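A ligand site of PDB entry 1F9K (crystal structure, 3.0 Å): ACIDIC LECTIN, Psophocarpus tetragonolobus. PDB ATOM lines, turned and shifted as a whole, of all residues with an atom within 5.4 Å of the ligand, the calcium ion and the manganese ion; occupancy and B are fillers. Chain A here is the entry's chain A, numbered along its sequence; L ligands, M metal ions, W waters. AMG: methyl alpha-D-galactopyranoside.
The nearest printed residue that does not touch the manganese ion is Ser 147 (4.1 Å).
The calcium ion is bound by water W3 (2.2 Å), water W5 (2.3 Å), OD2 of Asp 132 (2.3 Å), O of Phe 127 (2.4 Å), OD1 of Asn 129 (2.4 Å), OD1 of Asp 125 (2.4 Å) and OD2 of Asp 125 (2.6 Å).
Ala 87 touches the ligand (CB to O4, 3.8 Å).
Gly 105 touches the ligand (C to O3, 3.7 Å).
Gly 214 touches the ligand (CA to O4, 3.5 Å).
Ala 219 touches the ligand (CB to O6, 3.7 Å).
Hydrophobic or aromatic side chains that line the ligand: Ala 87, Phe 127, Tyr 215 and Ala 219.
Of the 23 residues printed, 10 come within 4 Å of the ligand.
The nearest printed residue that does not touch the ligand is Glu 85 (4.8 Å).
Water W1 lies within hydrogen-bond range of OE1 of Glu 123 (2.8 Å), O of Ile 145 (3.3 Å) and NE1 of Trp 131 (3.5 Å).
Water W2 lies within hydrogen-bond range of O6 of the ligand (2.6 Å) and O of Glu 85 (2.8 Å).
The manganese ion is bound by water W1, NE2 of His 137, OD1 of Asp 132, OD2 of Asp 125, OE2 of Glu 123 and water W4.
N of Gly 214 sits at hydrogen-bond distance from O of Ala 87, 3.5 Å away.
The backbone NH of Gly 106 sits at hydrogen-bond distance from the side-chain carboxylate of Asp 88, at 3.4 Å.
The backbone carbonyl oxygen (O) of Pro 133 lies within hydrogen-bond range of a ring nitrogen (ND1) of His 137 (3.4 Å).
The backbone carbonyl oxygen (O) of Asp 132 is in hydrogen-bond range of the side-chain amide nitrogen (NE2) of Gln 128 (3.1 Å).
N of Gly 214 sits at hydrogen-bond distance from O of Ala 219.
NE1 of Trp 131 sits close to OD1 of Asp 132 (3.2 Å).
ND2 of Asn 129 is in hydrogen-bond range of O3 of the ligand (3.4 Å).
The side-chain carboxylate (OD2) of Asp 88 sits at hydrogen-bond distance from an oxygen (O4) of the ligand (2.6 Å).
The side-chain amide nitrogen of Gln 216 lies within hydrogen-bond range of an oxygen (O6) of the ligand.
The backbone NH of Gly 106 lies within hydrogen-bond range of an oxygen (O3) of the ligand (2.8 Å).
An oxygen (O4) of the ligand lies within hydrogen-bond range of the backbone NH (N) of Tyr 215 (3.4 Å).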
ATOM      1  N   GLU A  85      13.387  34.322 -11.172  1.00  0.00           N
ATOM      2  CA  GLU A  85      12.223  34.204 -12.064  1.00  0.00           C
ATOM      3  C   GLU A  85      11.563  32.945 -11.514  1.00  0.00           C
ATOM      4  O   GLU A  85      12.074  31.858 -11.712  1.00  0.00           O
ATOM      5  CB  GLU A  85      12.696  33.973 -13.511  1.00  0.00           C
ATOM      6  CG  GLU A  85      11.744  34.511 -14.590  1.00  0.00           C
ATOM      7  CD  GLU A  85      12.399  34.711 -15.977  1.00  0.00           C
ATOM      8  OE1 GLU A  85      12.947  33.735 -16.550  1.00  0.00           O
ATOM      9  OE2 GLU A  85      12.358  35.839 -16.514  1.00  0.00           O
ATOM     10  N   ALA A  87       9.375  29.610 -10.353  1.00  0.00           N
ATOM     11  CA  ALA A  87       9.167  28.313 -10.992  1.00  0.00           C
ATOM     12  C   ALA A  87       8.669  27.357  -9.904  1.00  0.00           C
ATOM     13  O   ALA A  87       8.860  27.650  -8.733  1.00  0.00           O
ATOM     14  CB  ALA A  87      10.491  27.824 -11.612  1.00  0.00           C
ATOM     15  N   ASP A  88       8.044  26.237 -10.260  1.00  0.00           N
ATOM     16  CA  ASP A  88       7.784  25.852 -11.649  1.00  0.00           C
ATOM     17  C   ASP A  88       6.292  25.820 -11.942  1.00  0.00           C
ATOM     18  O   ASP A  88       5.888  26.031 -13.085  1.00  0.00           O
ATOM     19  CB  ASP A  88       8.374  24.470 -11.967  1.00  0.00           C
ATOM     20  CG  ASP A  88       9.815  24.538 -12.425  1.00  0.00           C
ATOM     21  OD1 ASP A  88      10.047  24.857 -13.612  1.00  0.00           O
ATOM     22  OD2 ASP A  88      10.721  24.292 -11.606  1.00  0.00           O
ATOM     23  N   GLY A 105      11.158  20.029 -11.021  1.00  0.00           N
ATOM     24  CA  GLY A 105      11.053  21.213 -11.861  1.00  0.00           C
ATOM     25  C   GLY A 105       9.996  21.247 -12.941  1.00  0.00           C
ATOM     26  O   GLY A 105       8.809  21.029 -12.682  1.00  0.00           O
ATOM     27  N   GLY A 106      10.444  21.525 -14.166  1.00  0.00           N
ATOM     28  CA  GLY A 106       9.570  21.632 -15.329  1.00  0.00           C
ATOM     29  C   GLY A 106       8.588  20.508 -15.580  1.00  0.00           C
ATOM     30  O   GLY A 106       7.620  20.692 -16.314  1.00  0.00           O
ATOM     31  N   ASN A 107       8.819  19.340 -15.003  1.00  0.00           N
ATOM     32  CA  ASN A 107       7.902  18.234 -15.177  1.00  0.00           C
ATOM     33  C   ASN A 107       6.829  18.199 -14.100  1.00  0.00           C
ATOM     34  O   ASN A 107       6.115  17.214 -13.944  1.00  0.00           O
ATOM     35  CB  ASN A 107       8.663  16.929 -15.253  1.00  0.00           C
ATOM     36  CG  ASN A 107       9.452  16.798 -16.540  1.00  0.00           C
ATOM     37  OD1 ASN A 107       8.870  16.590 -17.596  1.00  0.00           O
ATOM     38  ND2 ASN A 107      10.751  16.938 -16.446  1.00  0.00           N
ATOM     39  N   GLU A 123      -2.081  21.720 -16.060  1.00  0.00           N
ATOM     40  CA  GLU A 123      -1.073  22.556 -15.429  1.00  0.00           C
ATOM     41  C   GLU A 123      -1.317  24.051 -15.328  1.00  0.00           C
ATOM     42  O   GLU A 123      -2.078  24.661 -16.090  1.00  0.00           O
ATOM     43  CB  GLU A 123       0.275  22.333 -16.130  1.00  0.00           C
ATOM     44  CG  GLU A 123       0.230  22.683 -17.610  1.00  0.00           C
ATOM     45  CD  GLU A 123       1.593  22.650 -18.261  1.00  0.00           C
ATOM     46  OE1 GLU A 123       2.172  21.556 -18.406  1.00  0.00           O
ATOM     47  OE2 GLU A 123       2.072  23.723 -18.637  1.00  0.00           O
ATOM     48  N   ASP A 125       1.407  26.541 -15.271  1.00  0.00           N
ATOM     49  CA  ASP A 125       2.831  26.785 -15.476  1.00  0.00           C
ATOM     50  C   ASP A 125       3.245  28.217 -15.175  1.00  0.00           C
ATOM     51  O   ASP A 125       2.780  29.154 -15.806  1.00  0.00           O
ATOM     52  CB  ASP A 125       3.200  26.430 -16.920  1.00  0.00           C
ATOM     53  CG  ASP A 125       4.579  25.828 -17.040  1.00  0.00           C
ATOM     54  OD1 ASP A 125       5.452  26.150 -16.219  1.00  0.00           O
ATOM     55  OD2 ASP A 125       4.803  25.045 -17.981  1.00  0.00           O
ATOM     56  N   PHE A 127       6.725  28.913 -14.934  1.00  0.00           N
ATOM     57  CA  PHE A 127       8.065  29.037 -15.552  1.00  0.00           C
ATOM     58  C   PHE A 127       8.086  28.595 -17.007  1.00  0.00           C
ATOM     59  O   PHE A 127       7.595  27.517 -17.333  1.00  0.00           O
ATOM     60  CB  PHE A 127       9.077  28.194 -14.781  1.00  0.00           C
ATOM     61  CG  PHE A 127      10.490  28.420 -15.239  1.00  0.00           C
ATOM     62  CD1 PHE A 127      11.238  29.462 -14.714  1.00  0.00           C
ATOM     63  CD2 PHE A 127      11.054  27.628 -16.226  1.00  0.00           C
ATOM     64  CE1 PHE A 127      12.527  29.713 -15.177  1.00  0.00           C
ATOM     65  CE2 PHE A 127      12.321  27.881 -16.688  1.00  0.00           C
ATOM     66  CZ  PHE A 127      13.060  28.923 -16.175  1.00  0.00           C
ATOM     67  N   GLN A 128       8.693  29.406 -17.866  1.00  0.00           N
ATOM     68  CA  GLN A 128       8.773  29.078 -19.295  1.00  0.00           C
ATOM     69  C   GLN A 128       9.958  28.226 -19.680  1.00  0.00           C
ATOM     70  O   GLN A 128      11.079  28.720 -19.758  1.00  0.00           O
ATOM     71  CB  GLN A 128       8.810  30.350 -20.135  1.00  0.00           C
ATOM     72  CG  GLN A 128       9.111  30.112 -21.614  1.00  0.00           C
ATOM     73  CD  GLN A 128       8.889  31.347 -22.480  1.00  0.00           C
ATOM     74  OE1 GLN A 128       9.130  32.467 -22.050  1.00  0.00           O
ATOM     75  NE2 GLN A 128       8.435  31.146 -23.708  1.00  0.00           N
ATOM     76  N   ASN A 129       9.695  26.941 -19.920  1.00  0.00           N
ATOM     77  CA  ASN A 129      10.738  26.014 -20.332  1.00  0.00           C
ATOM     78  C   ASN A 129      10.947  26.209 -21.825  1.00  0.00           C
ATOM     79  O   ASN A 129      10.330  27.088 -22.435  1.00  0.00           O
ATOM     80  CB  ASN A 129      10.315  24.566 -20.061  1.00  0.00           C
ATOM     81  CG  ASN A 129      10.411  24.184 -18.581  1.00  0.00           C
ATOM     82  OD1 ASN A 129       9.621  24.640 -17.756  1.00  0.00           O
ATOM     83  ND2 ASN A 129      11.385  23.353 -18.259  1.00  0.00           N
ATOM     84  N   TRP A 131       9.988  24.389 -24.118  1.00  0.00           N
ATOM     85  CA  TRP A 131       8.817  23.900 -24.832  1.00  0.00           C
ATOM     86  C   TRP A 131       7.527  24.688 -24.513  1.00  0.00           C
ATOM     87  O   TRP A 131       6.475  24.356 -25.016  1.00  0.00           O
ATOM     88  CB  TRP A 131       8.595  22.427 -24.474  1.00  0.00           C
ATOM     89  CG  TRP A 131       8.376  22.211 -22.983  1.00  0.00           C
ATOM     90  CD1 TRP A 131       7.289  22.606 -22.237  1.00  0.00           C
ATOM     91  CD2 TRP A 131       9.268  21.579 -22.056  1.00  0.00           C
ATOM     92  NE1 TRP A 131       7.453  22.275 -20.912  1.00  0.00           N
ATOM     93  CE2 TRP A 131       8.658  21.636 -20.768  1.00  0.00           C
ATOM     94  CE3 TRP A 131      10.525  20.966 -22.175  1.00  0.00           C
ATOM     95  CZ2 TRP A 131       9.272  21.114 -19.624  1.00  0.00           C
ATOM     96  CZ3 TRP A 131      11.129  20.446 -21.042  1.00  0.00           C
ATOM     97  CH2 TRP A 131      10.502  20.524 -19.785  1.00  0.00           C
ATOM     98  N   ASP A 132       7.638  25.714 -23.657  1.00  0.00           N
ATOM     99  CA  ASP A 132       6.496  26.516 -23.210  1.00  0.00           C
ATOM    100  C   ASP A 132       6.264  27.823 -23.931  1.00  0.00           C
ATOM    101  O   ASP A 132       7.192  28.419 -24.477  1.00  0.00           O
ATOM    102  CB  ASP A 132       6.642  26.916 -21.724  1.00  0.00           C
ATOM    103  CG  ASP A 132       6.486  25.757 -20.774  1.00  0.00           C
ATOM    104  OD1 ASP A 132       5.644  24.885 -21.028  1.00  0.00           O
ATOM    105  OD2 ASP A 132       7.202  25.735 -19.757  1.00  0.00           O
ATOM    106  N   PRO A 133       5.000  28.304 -23.919  1.00  0.00           N
ATOM    107  CA  PRO A 133       4.587  29.568 -24.538  1.00  0.00           C
ATOM    108  C   PRO A 133       4.767  30.563 -23.401  1.00  0.00           C
ATOM    109  O   PRO A 133       5.121  30.172 -22.278  1.00  0.00           O
ATOM    110  CB  PRO A 133       3.110  29.331 -24.843  1.00  0.00           C
ATOM    111  CG  PRO A 133       2.938  27.820 -24.808  1.00  0.00           C
ATOM    112  CD  PRO A 133       3.830  27.442 -23.684  1.00  0.00           C
ATOM    113  N   HIS A 137       0.722  30.265 -17.767  1.00  0.00           N
ATOM    114  CA  HIS A 137      -0.346  29.763 -18.643  1.00  0.00           C
ATOM    115  C   HIS A 137      -0.959  28.481 -18.162  1.00  0.00           C
ATOM    116  O   HIS A 137      -0.346  27.702 -17.420  1.00  0.00           O
ATOM    117  CB  HIS A 137       0.159  29.534 -20.070  1.00  0.00           C
ATOM    118  CG  HIS A 137       1.280  28.541 -20.154  1.00  0.00           C
ATOM    119  ND1 HIS A 137       2.566  28.896 -20.475  1.00  0.00           N
ATOM    120  CD2 HIS A 137       1.310  27.222 -19.884  1.00  0.00           C
ATOM    121  CE1 HIS A 137       3.353  27.835 -20.395  1.00  0.00           C
ATOM    122  NE2 HIS A 137       2.613  26.803 -20.044  1.00  0.00           N
ATOM    123  N   ILE A 145       4.524  16.889 -21.155  1.00  0.00           N
ATOM    124  CA  ILE A 145       4.541  18.210 -20.538  1.00  0.00           C
ATOM    125  C   ILE A 145       4.181  19.227 -21.631  1.00  0.00           C
ATOM    126  O   ILE A 145       3.783  20.361 -21.338  1.00  0.00           O
ATOM    127  CB  ILE A 145       5.922  18.613 -19.972  1.00  0.00           C
ATOM    128  CG1 ILE A 145       7.038  18.092 -20.872  1.00  0.00           C
ATOM    129  CG2 ILE A 145       6.049  18.123 -18.545  1.00  0.00           C
ATOM    130  N   SER A 147       1.909  20.687 -23.456  1.00  0.00           N
ATOM    131  CA  SER A 147       0.475  20.883 -23.500  1.00  0.00           C
ATOM    132  C   SER A 147      -0.062  20.765 -24.911  1.00  0.00           C
ATOM    133  O   SER A 147       0.585  21.227 -25.843  1.00  0.00           O
ATOM    134  CB  SER A 147       0.108  22.251 -22.927  1.00  0.00           C
ATOM    135  OG  SER A 147       0.769  22.510 -21.701  1.00  0.00           O
ATOM    136  N   THR A 150      -2.828  25.588 -24.737  1.00  0.00           N
ATOM    137  CA  THR A 150      -2.496  26.456 -23.608  1.00  0.00           C
ATOM    138  C   THR A 150      -3.216  27.803 -23.693  1.00  0.00           C
ATOM    139  O   THR A 150      -3.690  28.188 -24.744  1.00  0.00           O
ATOM    140  CB  THR A 150      -0.963  26.775 -23.492  1.00  0.00           C
ATOM    141  OG1 THR A 150      -0.569  27.656 -24.555  1.00  0.00           O
ATOM    142  CG2 THR A 150      -0.140  25.509 -23.534  1.00  0.00           C
ATOM    143  N   THR A 213       9.175  23.540  -7.023  1.00  0.00           N
ATOM    144  CA  THR A 213       9.912  24.799  -7.045  1.00  0.00           C
ATOM    145  C   THR A 213      11.141  24.596  -7.923  1.00  0.00           C
ATOM    146  O   THR A 213      11.534  23.442  -8.185  1.00  0.00           O
ATOM    147  CB  THR A 213      10.327  25.282  -5.641  1.00  0.00           C
ATOM    148  OG1 THR A 213      11.148  24.301  -4.998  1.00  0.00           O
ATOM    149  CG2 THR A 213       9.094  25.568  -4.809  1.00  0.00           C
ATOM    150  N   GLY A 214      11.734  25.707  -8.364  1.00  0.00           N
ATOM    151  CA  GLY A 214      12.874  25.689  -9.270  1.00  0.00           C
ATOM    152  C   GLY A 214      14.187  24.965  -9.020  1.00  0.00           C
ATOM    153  O   GLY A 214      14.499  24.513  -7.923  1.00  0.00           O
ATOM    154  N   TYR A 215      14.958  24.855 -10.087  1.00  0.00           N
ATOM    155  CA  TYR A 215      16.245  24.195 -10.069  1.00  0.00           C
ATOM    156  C   TYR A 215      17.365  25.163  -9.717  1.00  0.00           C
ATOM    157  O   TYR A 215      18.522  24.801  -9.731  1.00  0.00           O
ATOM    158  CB  TYR A 215      16.557  23.594 -11.439  1.00  0.00           C
ATOM    159  CG  TYR A 215      16.379  22.107 -11.555  1.00  0.00           C
ATOM    160  CD1 TYR A 215      15.112  21.535 -11.491  1.00  0.00           C
ATOM    161  CD2 TYR A 215      17.460  21.277 -11.814  1.00  0.00           C
ATOM    162  CE1 TYR A 215      14.921  20.182 -11.695  1.00  0.00           C
ATOM    163  CE2 TYR A 215      17.291  19.922 -12.018  1.00  0.00           C
ATOM    164  CZ  TYR A 215      16.017  19.375 -11.964  1.00  0.00           C
ATOM    165  OH  TYR A 215      15.839  18.043 -12.243  1.00  0.00           O
ATOM    166  N   GLN A 216      17.020  26.395  -9.414  1.00  0.00           N
ATOM    167  CA  GLN A 216      18.050  27.358  -9.087  1.00  0.00           C
ATOM    168  C   GLN A 216      17.619  28.069  -7.812  1.00  0.00           C
ATOM    169  O   GLN A 216      16.443  28.173  -7.526  1.00  0.00           O
ATOM    170  CB  GLN A 216      18.216  28.345 -10.237  1.00  0.00           C
ATOM    171  CG  GLN A 216      18.092  27.670 -11.598  1.00  0.00           C
ATOM    172  CD  GLN A 216      18.741  28.447 -12.727  1.00  0.00           C
ATOM    173  OE1 GLN A 216      19.966  28.378 -12.922  1.00  0.00           O
ATOM    174  NE2 GLN A 216      17.941  29.199 -13.481  1.00  0.00           N
ATOM    175  N   ALA A 219      14.451  30.483  -7.355  1.00  0.00           N
ATOM    176  CA  ALA A 219      13.557  30.330  -8.506  1.00  0.00           C
ATOM    177  C   ALA A 219      12.389  29.509  -7.897  1.00  0.00           C
ATOM    178  O   ALA A 219      12.133  28.348  -8.244  1.00  0.00           O
ATOM    179  CB  ALA A 219      14.270  29.565  -9.588  1.00  0.00           C
HETATM  180  C1  AMG L   1      15.712  24.708 -15.025  1.00  0.00           C
HETATM  181  C2  AMG L   1      14.543  23.711 -14.950  1.00  0.00           C
HETATM  182  C3  AMG L   1      13.217  24.483 -15.110  1.00  0.00           C
HETATM  183  C4  AMG L   1      13.117  25.644 -14.084  1.00  0.00           C
HETATM  184  C5  AMG L   1      14.380  26.502 -14.083  1.00  0.00           C
HETATM  185  C6  AMG L   1      14.398  27.397 -12.864  1.00  0.00           C
HETATM  186  C7  AMG L   1      16.794  26.294 -16.450  1.00  0.00           C
HETATM  187  O1  AMG L   1      15.779  25.287 -16.291  1.00  0.00           O
HETATM  188  O2  AMG L   1      14.682  22.693 -15.941  1.00  0.00           O
HETATM  189  O3  AMG L   1      12.112  23.589 -14.941  1.00  0.00           O
HETATM  190  O4  AMG L   1      12.892  25.150 -12.769  1.00  0.00           O
HETATM  191  O5  AMG L   1      15.562  25.677 -13.991  1.00  0.00           O
HETATM  192  O6  AMG L   1      15.216  28.534 -13.067  1.00  0.00           O
HETATM  193 CA    CA M   1       7.303  25.184 -17.490  1.00  0.00          CA
HETATM  194 MN    MN M   2       3.648  24.814 -19.955  1.00  0.00          MN
HETATM  195  O   HOH W   1       4.432  22.886 -19.325  1.00  0.00           O
HETATM  196  O   HOH W   2      14.625  31.052 -12.651  1.00  0.00           O
HETATM  197  O   HOH W   3       6.773  23.035 -17.180  1.00  0.00           O
HETATM  198  O   HOH W   4       3.262  24.021 -22.143  1.00  0.00           O
HETATM  199  O   HOH W   5       7.662  25.024 -15.258  1.00  0.00           O
